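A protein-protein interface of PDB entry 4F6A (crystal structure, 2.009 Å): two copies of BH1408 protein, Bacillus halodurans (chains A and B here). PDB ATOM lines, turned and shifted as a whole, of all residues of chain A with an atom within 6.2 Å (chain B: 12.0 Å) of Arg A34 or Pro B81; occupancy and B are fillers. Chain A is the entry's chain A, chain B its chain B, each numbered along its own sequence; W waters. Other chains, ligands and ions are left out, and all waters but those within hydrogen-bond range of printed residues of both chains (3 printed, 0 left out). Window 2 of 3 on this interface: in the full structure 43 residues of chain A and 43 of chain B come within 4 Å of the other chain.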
ATOM      1  N   HIS A  22     -24.044  -5.020   9.554  1.00  0.00           N
ATOM      2  CA  HIS A  22     -23.942  -5.572   8.201  1.00  0.00           C
ATOM      3  C   HIS A  22     -25.204  -6.347   7.801  1.00  0.00           C
ATOM      4  O   HIS A  22     -25.725  -6.197   6.688  1.00  0.00           O
ATOM      5  CB  HIS A  22     -22.703  -6.469   8.058  1.00  0.00           C
ATOM      6  CG  HIS A  22     -22.478  -6.940   6.655  1.00  0.00           C
ATOM      7  ND1 HIS A  22     -21.948  -6.130   5.677  1.00  0.00           N
ATOM      8  CD2 HIS A  22     -22.764  -8.123   6.054  1.00  0.00           C
ATOM      9  CE1 HIS A  22     -21.886  -6.802   4.537  1.00  0.00           C
ATOM     10  NE2 HIS A  22     -22.377  -8.011   4.740  1.00  0.00           N
ATOM     11  N   GLU A  23     -25.705  -7.181   8.705  1.00  0.00           N
ATOM     12  CA  GLU A  23     -26.898  -7.951   8.377  1.00  0.00           C
ATOM     13  C   GLU A  23     -28.121  -7.063   8.163  1.00  0.00           C
ATOM     14  O   GLU A  23     -29.040  -7.427   7.415  1.00  0.00           O
ATOM     15  CB  GLU A  23     -27.156  -9.049   9.405  1.00  0.00           C
ATOM     16  CG  GLU A  23     -26.048 -10.154   9.407  1.00  0.00           C
ATOM     17  CD  GLU A  23     -25.843 -10.850   8.031  1.00  0.00           C
ATOM     18  OE1 GLU A  23     -26.815 -10.944   7.244  1.00  0.00           O
ATOM     19  OE2 GLU A  23     -24.701 -11.309   7.736  1.00  0.00           O
ATOM     20  N   VAL A  26     -27.642  -6.027   4.572  1.00  0.00           N
ATOM     21  CA  VAL A  26     -28.012  -7.158   3.723  1.00  0.00           C
ATOM     22  C   VAL A  26     -29.538  -7.231   3.566  1.00  0.00           C
ATOM     23  O   VAL A  26     -30.058  -7.440   2.466  1.00  0.00           O
ATOM     24  CB  VAL A  26     -27.493  -8.492   4.314  1.00  0.00           C
ATOM     25  CG1 VAL A  26     -28.096  -9.695   3.583  1.00  0.00           C
ATOM     26  CG2 VAL A  26     -25.957  -8.543   4.253  1.00  0.00           C
ATOM     27  N   ARG A  29     -30.642  -3.803   1.537  1.00  0.00           N
ATOM     28  CA  ARG A  29     -30.074  -3.662   0.200  1.00  0.00           C
ATOM     29  C   ARG A  29     -29.275  -4.914  -0.191  1.00  0.00           C
ATOM     30  O   ARG A  29     -28.069  -4.854  -0.399  1.00  0.00           O
ATOM     31  CB  ARG A  29     -29.191  -2.409   0.099  1.00  0.00           C
ATOM     32  CG  ARG A  29     -29.946  -1.063   0.215  1.00  0.00           C
ATOM     33  CD  ARG A  29     -30.972  -0.862  -0.901  1.00  0.00           C
ATOM     34  NE  ARG A  29     -30.412  -0.918  -2.256  1.00  0.00           N
ATOM     35  CZ  ARG A  29     -30.120   0.152  -2.998  1.00  0.00           C
ATOM     36  NH1 ARG A  29     -30.319   1.379  -2.520  1.00  0.00           N
ATOM     37  NH2 ARG A  29     -29.647  -0.001  -4.227  1.00  0.00           N
ATOM     38  N   GLY A  30     -29.961  -6.044  -0.306  1.00  0.00           N
ATOM     39  CA  GLY A  30     -29.306  -7.285  -0.682  1.00  0.00           C
ATOM     40  C   GLY A  30     -28.766  -7.269  -2.103  1.00  0.00           C
ATOM     41  O   GLY A  30     -28.031  -8.170  -2.499  1.00  0.00           O
ATOM     42  N   ILE A  32     -26.771  -5.038  -3.024  1.00  0.00           N
ATOM     43  CA  ILE A  32     -25.422  -4.509  -2.838  1.00  0.00           C
ATOM     44  C   ILE A  32     -24.621  -5.330  -1.825  1.00  0.00           C
ATOM     45  O   ILE A  32     -23.474  -5.693  -2.088  1.00  0.00           O
ATOM     46  CB  ILE A  32     -25.470  -3.026  -2.401  1.00  0.00           C
ATOM     47  CG1 ILE A  32     -26.050  -2.157  -3.525  1.00  0.00           C
ATOM     48  CG2 ILE A  32     -24.086  -2.517  -1.994  1.00  0.00           C
ATOM     49  CD1 ILE A  32     -26.337  -0.728  -3.087  1.00  0.00           C
ATOM     50  N   PHE A  33     -25.238  -5.627  -0.679  1.00  0.00           N
ATOM     51  CA  PHE A  33     -24.574  -6.340   0.418  1.00  0.00           C
ATOM     52  C   PHE A  33     -24.866  -7.843   0.461  1.00  0.00           C
ATOM     53  O   PHE A  33     -25.979  -8.280   0.165  1.00  0.00           O
ATOM     54  CB  PHE A  33     -24.957  -5.715   1.769  1.00  0.00           C
ATOM     55  CG  PHE A  33     -24.587  -4.264   1.889  1.00  0.00           C
ATOM     56  CD1 PHE A  33     -25.473  -3.272   1.478  1.00  0.00           C
ATOM     57  CD2 PHE A  33     -23.360  -3.890   2.413  1.00  0.00           C
ATOM     58  CE1 PHE A  33     -25.138  -1.928   1.586  1.00  0.00           C
ATOM     59  CE2 PHE A  33     -23.019  -2.537   2.534  1.00  0.00           C
ATOM     60  CZ  PHE A  33     -23.906  -1.561   2.116  1.00  0.00           C
ATOM     61  N   ARG A  34     -23.856  -8.611   0.872  1.00  0.00           N
ATOM     62  CA  ARG A  34     -23.907 -10.065   0.910  1.00  0.00           C
ATOM     63  C   ARG A  34     -23.614 -10.559   2.334  1.00  0.00           C
ATOM     64  O   ARG A  34     -22.744 -10.005   3.028  1.00  0.00           O
ATOM     65  CB  ARG A  34     -22.863 -10.621  -0.067  1.00  0.00           C
ATOM     66  CG  ARG A  34     -22.823 -12.134  -0.214  1.00  0.00           C
ATOM     67  CD  ARG A  34     -21.672 -12.570  -1.145  1.00  0.00           C
ATOM     68  NE  ARG A  34     -21.561 -14.026  -1.286  1.00  0.00           N
ATOM     69  CZ  ARG A  34     -20.952 -14.840  -0.415  1.00  0.00           C
ATOM     70  NH1 ARG A  34     -20.385 -14.363   0.695  1.00  0.00           N
ATOM     71  NH2 ARG A  34     -20.920 -16.147  -0.650  1.00  0.00           N
ATOM     72  N   SER A  35     -24.344 -11.580   2.776  1.00  0.00           N
ATOM     73  CA  SER A  35     -24.103 -12.189   4.083  1.00  0.00           C
ATOM     74  C   SER A  35     -22.837 -13.043   4.054  1.00  0.00           C
ATOM     75  O   SER A  35     -22.506 -13.646   3.032  1.00  0.00           O
ATOM     76  CB  SER A  35     -25.278 -13.079   4.499  1.00  0.00           C
ATOM     77  OG  SER A  35     -26.367 -12.310   4.987  1.00  0.00           O
ATOM     78  N   ASN A  36     -22.146 -13.121   5.188  1.00  0.00           N
ATOM     79  CA  ASN A  36     -20.963 -13.979   5.297  1.00  0.00           C
ATOM     80  C   ASN A  36     -20.625 -14.183   6.771  1.00  0.00           C
ATOM     81  O   ASN A  36     -21.037 -13.394   7.617  1.00  0.00           O
ATOM     82  CB  ASN A  36     -19.779 -13.343   4.565  1.00  0.00           C
ATOM     83  CG  ASN A  36     -18.691 -14.341   4.238  1.00  0.00           C
ATOM     84  OD1 ASN A  36     -18.816 -15.114   3.293  1.00  0.00           O
ATOM     85  ND2 ASN A  36     -17.612 -14.329   5.019  1.00  0.00           N
ATOM     86  N   PRO A  38     -17.136 -14.689   8.856  1.00  0.00           N
ATOM     87  CA  PRO A  38     -17.566 -13.470   9.551  1.00  0.00           C
ATOM     88  C   PRO A  38     -17.934 -12.370   8.570  1.00  0.00           C
ATOM     89  O   PRO A  38     -17.695 -12.534   7.381  1.00  0.00           O
ATOM     90  CB  PRO A  38     -16.299 -13.053  10.298  1.00  0.00           C
ATOM     91  CG  PRO A  38     -15.198 -13.467   9.372  1.00  0.00           C
ATOM     92  CD  PRO A  38     -15.663 -14.784   8.781  1.00  0.00           C
ATOM     93  N   THR A  39     -18.500 -11.267   9.054  1.00  0.00           N
ATOM     94  CA  THR A  39     -18.696 -10.109   8.191  1.00  0.00           C
ATOM     95  C   THR A  39     -17.503  -9.172   8.282  1.00  0.00           C
ATOM     96  O   THR A  39     -17.257  -8.391   7.374  1.00  0.00           O
ATOM     97  CB  THR A  39     -19.995  -9.343   8.504  1.00  0.00           C
ATOM     98  OG1 THR A  39     -19.920  -8.776   9.818  1.00  0.00           O
ATOM     99  CG2 THR A  39     -21.195 -10.280   8.419  1.00  0.00           C
ATOM    100  N   THR B  77     -17.342  -4.144 -10.056  1.00  0.00           N
ATOM    101  CA  THR B  77     -16.739  -4.727  -8.868  1.00  0.00           C
ATOM    102  C   THR B  77     -17.052  -6.217  -8.821  1.00  0.00           C
ATOM    103  O   THR B  77     -18.145  -6.647  -9.201  1.00  0.00           O
ATOM    104  CB  THR B  77     -17.237  -4.050  -7.588  1.00  0.00           C
ATOM    105  OG1 THR B  77     -18.612  -4.383  -7.378  1.00  0.00           O
ATOM    106  CG2 THR B  77     -17.091  -2.537  -7.699  1.00  0.00           C
ATOM    107  N   PRO B  78     -16.089  -7.017  -8.360  1.00  0.00           N
ATOM    108  CA  PRO B  78     -16.272  -8.467  -8.379  1.00  0.00           C
ATOM    109  C   PRO B  78     -17.022  -8.954  -7.146  1.00  0.00           C
ATOM    110  O   PRO B  78     -17.162  -8.205  -6.175  1.00  0.00           O
ATOM    111  CB  PRO B  78     -14.834  -8.980  -8.328  1.00  0.00           C
ATOM    112  CG  PRO B  78     -14.138  -7.965  -7.472  1.00  0.00           C
ATOM    113  CD  PRO B  78     -14.776  -6.633  -7.808  1.00  0.00           C
ATOM    114  N   LEU B  79     -17.491 -10.197  -7.193  1.00  0.00           N
ATOM    115  CA  LEU B  79     -18.074 -10.842  -6.024  1.00  0.00           C
ATOM    116  C   LEU B  79     -17.066 -10.870  -4.872  1.00  0.00           C
ATOM    117  O   LEU B  79     -15.932 -11.326  -5.035  1.00  0.00           O
ATOM    118  CB  LEU B  79     -18.509 -12.268  -6.371  1.00  0.00           C
ATOM    119  CG  LEU B  79     -19.196 -13.073  -5.266  1.00  0.00           C
ATOM    120  CD1 LEU B  79     -20.531 -12.441  -4.865  1.00  0.00           C
ATOM    121  CD2 LEU B  79     -19.379 -14.533  -5.691  1.00  0.00           C
ATOM    122  N   LEU B  80     -17.480 -10.364  -3.716  1.00  0.00           N
ATOM    123  CA  LEU B  80     -16.654 -10.400  -2.514  1.00  0.00           C
ATOM    124  C   LEU B  80     -17.424 -11.133  -1.419  1.00  0.00           C
ATOM    125  O   LEU B  80     -18.623 -11.386  -1.571  1.00  0.00           O
ATOM    126  CB  LEU B  80     -16.301  -8.979  -2.072  1.00  0.00           C
ATOM    127  CG  LEU B  80     -15.517  -8.138  -3.079  1.00  0.00           C
ATOM    128  CD1 LEU B  80     -15.271  -6.736  -2.526  1.00  0.00           C
ATOM    129  CD2 LEU B  80     -14.206  -8.813  -3.448  1.00  0.00           C
ATOM    130  N   PRO B  81     -16.743 -11.504  -0.321  1.00  0.00           N
ATOM    131  CA  PRO B  81     -17.463 -12.168   0.772  1.00  0.00           C
ATOM    132  C   PRO B  81     -18.670 -11.378   1.280  1.00  0.00           C
ATOM    133  O   PRO B  81     -19.708 -11.977   1.552  1.00  0.00           O
ATOM    134  CB  PRO B  81     -16.397 -12.278   1.865  1.00  0.00           C
ATOM    135  CG  PRO B  81     -15.122 -12.453   1.092  1.00  0.00           C
ATOM    136  CD  PRO B  81     -15.278 -11.590  -0.144  1.00  0.00           C
ATOM    137  N   THR B  82     -18.551 -10.059   1.376  1.00  0.00           N
ATOM    138  CA  THR B  82     -19.613  -9.250   1.971  1.00  0.00           C
ATOM    139  C   THR B  82     -20.291  -8.262   1.015  1.00  0.00           C
ATOM    140  O   THR B  82     -21.121  -7.459   1.448  1.00  0.00           O
ATOM    141  CB  THR B  82     -19.104  -8.467   3.196  1.00  0.00           C
ATOM    142  OG1 THR B  82     -18.029  -7.610   2.801  1.00  0.00           O
ATOM    143  CG2 THR B  82     -18.618  -9.426   4.295  1.00  0.00           C
ATOM    144  N   MET B  83     -19.939  -8.316  -0.269  1.00  0.00           N
ATOM    145  CA  MET B  83     -20.529  -7.424  -1.267  1.00  0.00           C
ATOM    146  C   MET B  83     -20.893  -8.182  -2.539  1.00  0.00           C
ATOM    147  O   MET B  83     -20.105  -8.986  -3.042  1.00  0.00           O
ATOM    148  CB  MET B  83     -19.560  -6.294  -1.621  1.00  0.00           C
ATOM    149  CG  MET B  83     -19.135  -5.443  -0.441  1.00  0.00           C
ATOM    150  SD  MET B  83     -20.630  -4.450   0.354  1.00  0.00           S
ATOM    151  CE  MET B  83     -20.596  -2.868  -0.803  1.00  0.00           C
ATOM    152  N   GLN B  84     -22.085  -7.930  -3.068  1.00  0.00           N
ATOM    153  CA  GLN B  84     -22.479  -8.554  -4.333  1.00  0.00           C
ATOM    154  C   GLN B  84     -21.623  -8.036  -5.483  1.00  0.00           C
ATOM    155  O   GLN B  84     -21.117  -6.915  -5.436  1.00  0.00           O
ATOM    156  CB  GLN B  84     -23.954  -8.281  -4.647  1.00  0.00           C
ATOM    157  CG  GLN B  84     -24.921  -8.653  -3.535  1.00  0.00           C
ATOM    158  CD  GLN B  84     -25.075 -10.160  -3.361  1.00  0.00           C
ATOM    159  OE1 GLN B  84     -24.478 -10.946  -4.090  1.00  0.00           O
ATOM    160  NE2 GLN B  84     -25.873 -10.562  -2.379  1.00  0.00           N
ATOM    161  N   GLN B  85     -21.468  -8.861  -6.513  1.00  0.00           N
ATOM    162  CA  GLN B  85     -20.884  -8.403  -7.763  1.00  0.00           C
ATOM    163  C   GLN B  85     -21.802  -7.316  -8.318  1.00  0.00           C
ATOM    164  O   GLN B  85     -23.020  -7.436  -8.228  1.00  0.00           O
ATOM    165  CB  GLN B  85     -20.773  -9.568  -8.744  1.00  0.00           C
ATOM    166  CG  GLN B  85     -20.347  -9.166 -10.142  1.00  0.00           C
ATOM    167  CD  GLN B  85     -20.083 -10.363 -11.037  1.00  0.00           C
ATOM    168  OE1 GLN B  85     -19.772 -11.455 -10.556  1.00  0.00           O
ATOM    169  NE2 GLN B  85     -20.205 -10.163 -12.348  1.00  0.00           N
ATOM    170  N   ARG B  86     -21.226  -6.249  -8.861  1.00  0.00           N
ATOM    171  CA  ARG B  86     -22.027  -5.108  -9.298  1.00  0.00           C
ATOM    172  C   ARG B  86     -21.394  -4.422 -10.505  1.00  0.00           C
ATOM    173  O   ARG B  86     -20.185  -4.201 -10.546  1.00  0.00           O
ATOM    174  CB  ARG B  86     -22.190  -4.117  -8.140  1.00  0.00           C
ATOM    175  CG  ARG B  86     -23.238  -3.039  -8.346  1.00  0.00           C
ATOM    176  CD  ARG B  86     -23.620  -2.370  -7.019  1.00  0.00           C
ATOM    177  NE  ARG B  86     -24.342  -1.111  -7.226  1.00  0.00           N
ATOM    178  CZ  ARG B  86     -25.629  -1.039  -7.529  1.00  0.00           C
ATOM    179  NH1 ARG B  86     -26.338  -2.155  -7.648  1.00  0.00           N
ATOM    180  NH2 ARG B  86     -26.206   0.142  -7.714  1.00  0.00           N
HETATM  181  O   HOH W   1     -21.984  -4.571  -4.269  1.00  0.00           O
HETATM  182  O   HOH W   2     -27.792 -10.553  -0.272  1.00  0.00           O
HETATM  183  O   HOH W   3     -23.873 -13.656  -3.481  1.00  0.00           O
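No position is printed for both chains.
Among the printed residues, merely in contact across the chains: His A22 with Thr B82 (3.2 Å), Ile A32 with Met B83 (3.5 Å), Phe A33 with Thr B82 (3.8 Å), Phe A33 with Met B83 (3.5 Å), Arg A34 with Leu B79 (3.9 Å), Arg A34 with Leu B80 (3.3 Å), Arg A34 with Met B83 (3.7 Å), Arg A34 with Gln B84 (3.8 Å), Ser A35 with Pro B81 (3.6 Å), Asn A36 with Pro B81 (3.3 Å) and Thr A39 with Thr B82 (3.5 Å).
Water W1 bridges O of Gln B84 and O of Ile A32. Water W3 bridges the side-chain amide oxygen of Gln B84 and the guanidinium group of Arg A34. Water W2 lies within hydrogen-bond range of NE2 of Gln B84 (2.8 Å), O of Phe A33 (2.9 Å) and O of Gly A30 (3.3 Å).
Hydrophobic or aromatic side chains of chain A within 4 Å of the printed part of chain B: His A22, Ile A32 and Phe A33. Of the 10 printed residues of chain B, 6 touch a printed residue of chain A. Hydrophobic or aromatic side chains of chain B that line the printed part of chain A: Leu B79, Pro B81 and Met B83. Among the printed residues, 16 pairs touch across the chains. Among the printed residues, no Asp or Glu carboxylate lies within 4 Å of a Lys or Arg side-chain nitrogen of the other chain.
O of Phe A33 sits at hydrogen-bond distance from NE2 of Gln B84 (3.4 Å). The backbone carbonyl oxygen (O) of Ile A32 lies within hydrogen-bond range of the backbone NH (N) of Gln B84. The backbone carbonyl oxygen of Gly A30 lies within hydrogen-bond range of the side-chain amide nitrogen of Gln B84 (3.2 Å). The guanidinium group (NH1) of Arg A34 sits at hydrogen-bond distance from the backbone carbonyl oxygen (O) of Pro B81 (2.6 Å). The backbone NH (N) of Arg A34 lies within hydrogen-bond range of the backbone carbonyl oxygen (O) of Thr B82, 3.0 Å away.
Of chain B, only Leu B79, Leu B80, Pro B81, Thr B82, Met B83 and Gln B84 come within 4 Å of Arg A34. Of chain B, only Gln B84 comes within 4 Å of Gly A30. Printed residues of chain B within 4 Å of Ser A35: Pro B81 (3.6 Å). Asn A36 touches just one residue of chain B: Pro B81 (3.3 Å). Thr A39 touches just one residue of chain B: Thr B82. Of the printed residues of chain A, Leu B79 touches Arg A34 (3.9 Å). Printed residues of chain A within 4 Å of Leu B80: Arg A34. Printed residues of chain A within 4 Å of Met B83: Ile A32 (3.5 Å), Phe A33 (3.5 Å) and Arg A34 (3.7 Å). Pro B78 touches none of the printed residues of chain A. Glu A23 touches none of the printed residues of chain B. The nearest residue of chain B that does not touch Arg A34 is Gln B85 (6.5 Å). The nearest residue of chain A that does not touch Pro B81 is Pro A38 (5.7 Å).
The side-chain carboxylate (OE1) of Glu A23 sits at hydrogen-bond distance from the side-chain hydroxyl (OG) of Ser A35 (2.7 Å). The guanidinium group (NH1) of Arg A34 lies within hydrogen-bond range of the side-chain amide oxygen (OD1) of Asn A36, at 3.1 Å. A ring nitrogen (NE2) of His A22 lies within hydrogen-bond range of the backbone carbonyl oxygen (O) of Arg A34 (2.7 Å). O of Pro A38 is in hydrogen-bond range of ND2 of Asn A36 (3.0 Å).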
